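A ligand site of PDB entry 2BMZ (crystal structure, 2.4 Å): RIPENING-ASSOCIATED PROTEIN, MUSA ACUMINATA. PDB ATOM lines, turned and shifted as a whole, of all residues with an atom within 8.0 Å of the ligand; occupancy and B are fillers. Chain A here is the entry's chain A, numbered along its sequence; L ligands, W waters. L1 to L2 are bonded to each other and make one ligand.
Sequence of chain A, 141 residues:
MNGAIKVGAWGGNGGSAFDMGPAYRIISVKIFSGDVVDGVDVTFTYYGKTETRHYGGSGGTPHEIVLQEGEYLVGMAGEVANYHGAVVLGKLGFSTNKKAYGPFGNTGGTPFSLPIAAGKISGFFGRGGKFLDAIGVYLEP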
ATOM      1  N   PHE A  32     -19.235 -21.882  -2.819  1.00  0.00           N
ATOM      2  CA  PHE A  32     -18.855 -23.183  -3.344  1.00  0.00           C
ATOM      3  C   PHE A  32     -20.018 -23.802  -4.101  1.00  0.00           C
ATOM      4  O   PHE A  32     -21.072 -24.098  -3.517  1.00  0.00           O
ATOM      5  CB  PHE A  32     -18.393 -24.115  -2.217  1.00  0.00           C
ATOM      6  CG  PHE A  32     -17.019 -23.794  -1.691  1.00  0.00           C
ATOM      7  CD1 PHE A  32     -16.796 -22.632  -0.953  1.00  0.00           C
ATOM      8  CD2 PHE A  32     -15.942 -24.631  -1.978  1.00  0.00           C
ATOM      9  CE1 PHE A  32     -15.509 -22.312  -0.508  1.00  0.00           C
ATOM     10  CE2 PHE A  32     -14.658 -24.310  -1.542  1.00  0.00           C
ATOM     11  CZ  PHE A  32     -14.436 -23.148  -0.804  1.00  0.00           C
ATOM     12  N   SER A  33     -19.818 -24.037  -5.392  1.00  0.00           N
ATOM     13  CA  SER A  33     -20.875 -24.597  -6.228  1.00  0.00           C
ATOM     14  C   SER A  33     -20.487 -25.730  -7.180  1.00  0.00           C
ATOM     15  O   SER A  33     -19.324 -25.901  -7.545  1.00  0.00           O
ATOM     16  CB  SER A  33     -21.494 -23.484  -7.066  1.00  0.00           C
ATOM     17  OG  SER A  33     -20.502 -22.883  -7.872  1.00  0.00           O
ATOM     18  N   GLY A  34     -21.512 -26.460  -7.586  1.00  0.00           N
ATOM     19  CA  GLY A  34     -21.384 -27.564  -8.527  1.00  0.00           C
ATOM     20  C   GLY A  34     -22.690 -27.573  -9.292  1.00  0.00           C
ATOM     21  O   GLY A  34     -22.977 -26.651 -10.059  1.00  0.00           O
ATOM     22  N   ASP A  35     -23.499 -28.604  -9.083  1.00  0.00           N
ATOM     23  CA  ASP A  35     -24.797 -28.652  -9.743  1.00  0.00           C
ATOM     24  C   ASP A  35     -25.617 -27.570  -9.036  1.00  0.00           C
ATOM     25  O   ASP A  35     -26.396 -26.837  -9.661  1.00  0.00           O
ATOM     26  CB  ASP A  35     -25.464 -30.017  -9.536  1.00  0.00           C
ATOM     27  CG  ASP A  35     -24.692 -31.164 -10.191  1.00  0.00           C
ATOM     28  OD1 ASP A  35     -23.976 -30.914 -11.182  1.00  0.00           O
ATOM     29  OD2 ASP A  35     -24.822 -32.310  -9.704  1.00  0.00           O
ATOM     30  N   VAL A  36     -25.416 -27.471  -7.725  1.00  0.00           N
ATOM     31  CA  VAL A  36     -26.119 -26.517  -6.889  1.00  0.00           C
ATOM     32  C   VAL A  36     -25.077 -25.765  -6.049  1.00  0.00           C
ATOM     33  O   VAL A  36     -23.877 -25.838  -6.318  1.00  0.00           O
ATOM     34  CB  VAL A  36     -27.083 -27.246  -5.957  1.00  0.00           C
ATOM     35  CG1 VAL A  36     -28.003 -28.139  -6.771  1.00  0.00           C
ATOM     36  CG2 VAL A  36     -26.314 -28.078  -4.946  1.00  0.00           C
ATOM     37  N   VAL A  37     -25.556 -25.030  -5.050  1.00  0.00           N
ATOM     38  CA  VAL A  37     -24.639 -24.300  -4.175  1.00  0.00           C
ATOM     39  C   VAL A  37     -24.378 -25.222  -2.989  1.00  0.00           C
ATOM     40  O   VAL A  37     -25.309 -25.669  -2.303  1.00  0.00           O
ATOM     41  CB  VAL A  37     -25.239 -22.960  -3.679  1.00  0.00           C
ATOM     42  CG1 VAL A  37     -24.200 -22.222  -2.839  1.00  0.00           C
ATOM     43  CG2 VAL A  37     -25.646 -22.109  -4.868  1.00  0.00           C
ATOM     44  N   ASP A  38     -23.109 -25.504  -2.747  1.00  0.00           N
ATOM     45  CA  ASP A  38     -22.707 -26.397  -1.669  1.00  0.00           C
ATOM     46  C   ASP A  38     -22.615 -25.714  -0.328  1.00  0.00           C
ATOM     47  O   ASP A  38     -23.183 -26.178   0.663  1.00  0.00           O
ATOM     48  CB  ASP A  38     -21.368 -27.040  -2.025  1.00  0.00           C
ATOM     49  CG  ASP A  38     -21.488 -28.024  -3.166  1.00  0.00           C
ATOM     50  OD1 ASP A  38     -21.867 -29.194  -2.907  1.00  0.00           O
ATOM     51  OD2 ASP A  38     -21.223 -27.634  -4.319  1.00  0.00           O
ATOM     52  N   GLY A  39     -21.877 -24.605  -0.304  1.00  0.00           N
ATOM     53  CA  GLY A  39     -21.714 -23.886   0.929  1.00  0.00           C
ATOM     54  C   GLY A  39     -21.176 -22.496   0.672  1.00  0.00           C
ATOM     55  O   GLY A  39     -20.907 -22.107  -0.472  1.00  0.00           O
ATOM     56  N   GLY A  57     -22.491 -27.341   2.908  1.00  0.00           N
ATOM     57  CA  GLY A  57     -21.656 -28.515   2.773  1.00  0.00           C
ATOM     58  C   GLY A  57     -20.223 -28.181   2.381  1.00  0.00           C
ATOM     59  O   GLY A  57     -19.879 -27.021   2.171  1.00  0.00           O
ATOM     60  N   SER A  58     -19.403 -29.219   2.281  1.00  0.00           N
ATOM     61  CA  SER A  58     -17.980 -29.061   1.941  1.00  0.00           C
ATOM     62  C   SER A  58     -17.616 -29.256   0.466  1.00  0.00           C
ATOM     63  O   SER A  58     -16.491 -28.964   0.070  1.00  0.00           O
ATOM     64  CB  SER A  58     -17.148 -30.024   2.797  1.00  0.00           C
ATOM     65  OG  SER A  58     -17.728 -31.328   2.768  1.00  0.00           O
ATOM     66  N   GLY A  59     -18.562 -29.728  -0.330  1.00  0.00           N
ATOM     67  CA  GLY A  59     -18.294 -29.949  -1.740  1.00  0.00           C
ATOM     68  C   GLY A  59     -18.186 -28.704  -2.598  1.00  0.00           C
ATOM     69  O   GLY A  59     -17.973 -27.597  -2.089  1.00  0.00           O
ATOM     70  N   GLY A  60     -18.314 -28.891  -3.913  1.00  0.00           N
ATOM     71  CA  GLY A  60     -18.260 -27.792  -4.862  1.00  0.00           C
ATOM     72  C   GLY A  60     -16.948 -27.059  -5.073  1.00  0.00           C
ATOM     73  O   GLY A  60     -15.959 -27.290  -4.381  1.00  0.00           O
ATOM     74  N   THR A  61     -16.965 -26.157  -6.053  1.00  0.00           N
ATOM     75  CA  THR A  61     -15.824 -25.339  -6.434  1.00  0.00           C
ATOM     76  C   THR A  61     -15.974 -23.944  -5.824  1.00  0.00           C
ATOM     77  O   THR A  61     -17.098 -23.447  -5.683  1.00  0.00           O
ATOM     78  CB  THR A  61     -15.756 -25.175  -7.957  1.00  0.00           C
ATOM     79  OG1 THR A  61     -15.757 -26.478  -8.560  1.00  0.00           O
ATOM     80  CG2 THR A  61     -14.505 -24.412  -8.381  1.00  0.00           C
ATOM     81  N   PRO A  62     -14.853 -23.289  -5.465  1.00  0.00           N
ATOM     82  CA  PRO A  62     -14.916 -21.950  -4.864  1.00  0.00           C
ATOM     83  C   PRO A  62     -14.966 -20.780  -5.851  1.00  0.00           C
ATOM     84  O   PRO A  62     -14.293 -20.776  -6.887  1.00  0.00           O
ATOM     85  CB  PRO A  62     -13.665 -21.916  -4.006  1.00  0.00           C
ATOM     86  CG  PRO A  62     -12.681 -22.644  -4.874  1.00  0.00           C
ATOM     87  CD  PRO A  62     -13.497 -23.851  -5.352  1.00  0.00           C
ATOM     88  N   TYR A  83     -33.412 -31.076  -5.503  1.00  0.00           N
ATOM     89  CA  TYR A  83     -32.159 -31.709  -5.863  1.00  0.00           C
ATOM     90  C   TYR A  83     -32.114 -32.982  -5.054  1.00  0.00           C
ATOM     91  O   TYR A  83     -31.916 -32.961  -3.845  1.00  0.00           O
ATOM     92  CB  TYR A  83     -30.971 -30.820  -5.481  1.00  0.00           C
ATOM     93  CG  TYR A  83     -29.633 -31.299  -5.995  1.00  0.00           C
ATOM     94  CD1 TYR A  83     -29.305 -31.195  -7.343  1.00  0.00           C
ATOM     95  CD2 TYR A  83     -28.680 -31.830  -5.122  1.00  0.00           C
ATOM     96  CE1 TYR A  83     -28.046 -31.603  -7.806  1.00  0.00           C
ATOM     97  CE2 TYR A  83     -27.430 -32.236  -5.571  1.00  0.00           C
ATOM     98  CZ  TYR A  83     -27.116 -32.115  -6.922  1.00  0.00           C
ATOM     99  OH  TYR A  83     -25.870 -32.512  -7.369  1.00  0.00           O
ATOM    100  N   HIS A  84     -32.347 -34.110  -5.731  1.00  0.00           N
ATOM    101  CA  HIS A  84     -32.349 -35.419  -5.089  1.00  0.00           C
ATOM    102  C   HIS A  84     -33.268 -35.461  -3.875  1.00  0.00           C
ATOM    103  O   HIS A  84     -32.862 -35.898  -2.802  1.00  0.00           O
ATOM    104  CB  HIS A  84     -30.923 -35.805  -4.682  1.00  0.00           C
ATOM    105  CG  HIS A  84     -29.943 -35.743  -5.813  1.00  0.00           C
ATOM    106  ND1 HIS A  84     -30.267 -36.082  -7.110  1.00  0.00           N
ATOM    107  CD2 HIS A  84     -28.627 -35.398  -5.832  1.00  0.00           C
ATOM    108  CE1 HIS A  84     -29.202 -35.938  -7.880  1.00  0.00           C
ATOM    109  NE2 HIS A  84     -28.199 -35.524  -7.135  1.00  0.00           N
ATOM    110  N   VAL A  88     -32.927 -26.985  -2.167  1.00  0.00           N
ATOM    111  CA  VAL A  88     -31.743 -26.246  -1.768  1.00  0.00           C
ATOM    112  C   VAL A  88     -31.442 -25.170  -2.810  1.00  0.00           C
ATOM    113  O   VAL A  88     -32.128 -25.066  -3.812  1.00  0.00           O
ATOM    114  CB  VAL A  88     -30.520 -27.186  -1.675  1.00  0.00           C
ATOM    115  CG1 VAL A  88     -30.882 -28.438  -0.876  1.00  0.00           C
ATOM    116  CG2 VAL A  88     -30.035 -27.562  -3.070  1.00  0.00           C
ATOM    117  N   LEU A  89     -30.398 -24.381  -2.564  1.00  0.00           N
ATOM    118  CA  LEU A  89     -30.012 -23.338  -3.492  1.00  0.00           C
ATOM    119  C   LEU A  89     -29.309 -23.916  -4.709  1.00  0.00           C
ATOM    120  O   LEU A  89     -28.198 -24.434  -4.614  1.00  0.00           O
ATOM    121  CB  LEU A  89     -29.090 -22.323  -2.807  1.00  0.00           C
ATOM    122  CG  LEU A  89     -29.674 -21.264  -1.856  1.00  0.00           C
ATOM    123  CD1 LEU A  89     -30.595 -20.358  -2.651  1.00  0.00           C
ATOM    124  CD2 LEU A  89     -30.432 -21.939  -0.720  1.00  0.00           C
ATOM    125  N   GLY A  90     -29.956 -23.801  -5.872  1.00  0.00           N
ATOM    126  CA  GLY A  90     -29.366 -24.298  -7.100  1.00  0.00           C
ATOM    127  C   GLY A  90     -28.457 -23.272  -7.741  1.00  0.00           C
ATOM    128  O   GLY A  90     -27.569 -23.618  -8.516  1.00  0.00           O
ATOM    129  N   GLY A 105     -23.699 -21.966  -9.701  1.00  0.00           N
ATOM    130  CA  GLY A 105     -24.525 -23.146  -9.501  1.00  0.00           C
ATOM    131  C   GLY A 105     -25.106 -23.455 -10.866  1.00  0.00           C
ATOM    132  O   GLY A 105     -24.968 -22.640 -11.778  1.00  0.00           O
ATOM    133  N   ASN A 106     -25.777 -24.595 -11.022  1.00  0.00           N
ATOM    134  CA  ASN A 106     -26.325 -24.951 -12.326  1.00  0.00           C
ATOM    135  C   ASN A 106     -27.722 -25.561 -12.292  1.00  0.00           C
ATOM    136  O   ASN A 106     -28.279 -25.893 -13.338  1.00  0.00           O
ATOM    137  CB  ASN A 106     -25.367 -25.918 -13.038  1.00  0.00           C
ATOM    138  CG  ASN A 106     -23.992 -25.309 -13.271  1.00  0.00           C
ATOM    139  OD1 ASN A 106     -22.982 -25.872 -12.856  1.00  0.00           O
ATOM    140  ND2 ASN A 106     -23.965 -24.165 -13.943  1.00  0.00           N
ATOM    141  N   THR A 107     -28.285 -25.710 -11.114  1.00  0.00           N
ATOM    142  CA  THR A 107     -29.615 -26.271 -10.998  1.00  0.00           C
ATOM    143  C   THR A 107     -30.659 -25.149 -10.924  1.00  0.00           C
ATOM    144  O   THR A 107     -30.740 -24.428  -9.921  1.00  0.00           O
ATOM    145  CB  THR A 107     -29.735 -27.136  -9.767  1.00  0.00           C
ATOM    146  OG1 THR A 107     -28.615 -28.027  -9.713  1.00  0.00           O
ATOM    147  CG2 THR A 107     -31.032 -27.922  -9.786  1.00  0.00           C
ATOM    148  N   LYS A 130     -25.849 -31.174   3.504  1.00  0.00           N
ATOM    149  CA  LYS A 130     -24.838 -31.651   2.568  1.00  0.00           C
ATOM    150  C   LYS A 130     -24.580 -30.486   1.627  1.00  0.00           C
ATOM    151  O   LYS A 130     -23.483 -30.313   1.096  1.00  0.00           O
ATOM    152  CB  LYS A 130     -25.350 -32.875   1.807  1.00  0.00           C
ATOM    153  CG  LYS A 130     -24.345 -33.427   0.793  1.00  0.00           C
ATOM    154  CD  LYS A 130     -24.771 -34.787   0.251  1.00  0.00           C
ATOM    155  CE  LYS A 130     -23.896 -35.211  -0.918  1.00  0.00           C
ATOM    156  NZ  LYS A 130     -22.443 -35.071  -0.590  1.00  0.00           N
ATOM    157  N   PHE A 131     -25.621 -29.672   1.423  1.00  0.00           N
ATOM    158  CA  PHE A 131     -25.542 -28.479   0.565  1.00  0.00           C
ATOM    159  C   PHE A 131     -26.141 -27.284   1.308  1.00  0.00           C
ATOM    160  O   PHE A 131     -26.479 -27.380   2.495  1.00  0.00           O
ATOM    161  CB  PHE A 131     -26.314 -28.700  -0.742  1.00  0.00           C
ATOM    162  CG  PHE A 131     -25.997 -29.990  -1.424  1.00  0.00           C
ATOM    163  CD1 PHE A 131     -26.864 -31.073  -1.345  1.00  0.00           C
ATOM    164  CD2 PHE A 131     -24.802 -30.137  -2.124  1.00  0.00           C
ATOM    165  CE1 PHE A 131     -26.553 -32.292  -1.956  1.00  0.00           C
ATOM    166  CE2 PHE A 131     -24.475 -31.346  -2.742  1.00  0.00           C
ATOM    167  CZ  PHE A 131     -25.354 -32.426  -2.657  1.00  0.00           C
HETATM  168  C1  LIG L   1     -21.276 -32.270  -8.547  1.00  0.00           C
HETATM  169  C2  LIG L   1     -19.840 -31.725  -8.294  1.00  0.00           C
HETATM  170  C3  LIG L   1     -19.553 -31.618  -6.769  1.00  0.00           C
HETATM  171  C4  LIG L   1     -20.599 -30.730  -6.119  1.00  0.00           C
HETATM  172  C5  LIG L   1     -22.024 -31.272  -6.400  1.00  0.00           C
HETATM  173  C6  LIG L   1     -23.108 -30.373  -5.821  1.00  0.00           C
HETATM  174  C7  LIG L   1     -22.666 -34.227  -8.241  1.00  0.00           C
HETATM  175  O1  LIG L   1     -21.356 -33.593  -8.047  1.00  0.00           O
HETATM  176  O2  LIG L   1     -19.727 -30.419  -8.833  1.00  0.00           O
HETATM  177  O3  LIG L   1     -18.251 -30.991  -6.605  1.00  0.00           O
HETATM  178  O4  LIG L   1     -20.359 -30.620  -4.728  1.00  0.00           O
HETATM  179  O5  LIG L   1     -22.231 -31.392  -7.852  1.00  0.00           O
HETATM  180  O6  LIG L   1     -22.965 -29.033  -6.295  1.00  0.00           O
HETATM  181  C1  LG2 L   2     -17.279 -31.774  -6.004  1.00  0.00           C
HETATM  182  C2  LG2 L   2     -15.935 -31.024  -6.053  1.00  0.00           C
HETATM  183  C3  LG2 L   2     -14.863 -31.882  -5.369  1.00  0.00           C
HETATM  184  C4  LG2 L   2     -15.295 -32.160  -3.915  1.00  0.00           C
HETATM  185  C5  LG2 L   2     -16.675 -32.883  -3.904  1.00  0.00           C
HETATM  186  O1  LG2 L   2     -15.562 -30.764  -7.403  1.00  0.00           O
HETATM  187  O2  LG2 L   2     -13.603 -31.208  -5.404  1.00  0.00           O
HETATM  188  O3  LG2 L   2     -14.319 -32.948  -3.251  1.00  0.00           O
HETATM  189  O4  LG2 L   2     -17.675 -32.057  -4.622  1.00  0.00           O
HETATM  190  O   HOH W   1     -19.785 -29.462 -11.377  1.00  0.00           O
HETATM  191  O   HOH W   2     -17.654 -28.783  -8.762  1.00  0.00           O
HETATM  192  O   HOH W   3     -20.538 -33.289  -3.454  1.00  0.00           O
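OD1 of Asp 38 sits at hydrogen-bond distance from O4 of LIG L1 (2.8 Å).
N of Gly 60 is in hydrogen-bond range of O4 of LIG L1, at 2.8 Å.
N of Asp 35 lies within hydrogen-bond range of O6 of LIG L1, at 2.9 Å.
O6 of LIG L1 sits close to N of Gly 34, at 3.2 Å.
The backbone NH (N) of Val 36 is in hydrogen-bond range of an oxygen (O6) of LIG L1 (3.2 Å).
O of Val 36 lies within hydrogen-bond range of O6 of LIG L1 (3.3 Å).
The backbone NH (N) of Gly 60 sits close to the side-chain carboxylate (OD2) of Asp 38, 3.2 Å away.
OD2 of Asp 38 is in hydrogen-bond range of N of Gly 34 (3.5 Å).
The backbone NH (N) of Asp 38 is in hydrogen-bond range of the backbone carbonyl oxygen (O) of Phe 32 (2.6 Å).
N of Gly 57 sits at hydrogen-bond distance from O of Asp 38 (2.6 Å).
The side-chain carboxylate (OD2) of Asp 35 sits at hydrogen-bond distance from the side-chain hydroxyl (OH) of Tyr 83, at 2.6 Å.
The backbone carbonyl oxygen of Asp 35 sits at hydrogen-bond distance from the side-chain hydroxyl of Thr 107.
N of Asn 106 sits at hydrogen-bond distance from O of Asp 35 (2.7 Å).
O of Gly 34 lies close to OD1 of Asn 106 (2.9 Å).
Gly 59 touches the ligand.
OH of Tyr 83 touches C7 of LIG L1 (3.7 Å).
Phe 131 touches the ligand.
Along chain A the residues within 4 Å of the ligand span positions 34 to 131.
Water W2 lies within hydrogen-bond range of O2 of LIG L1 (2.6 Å) and OG1 of Thr 61 (3.0 Å).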
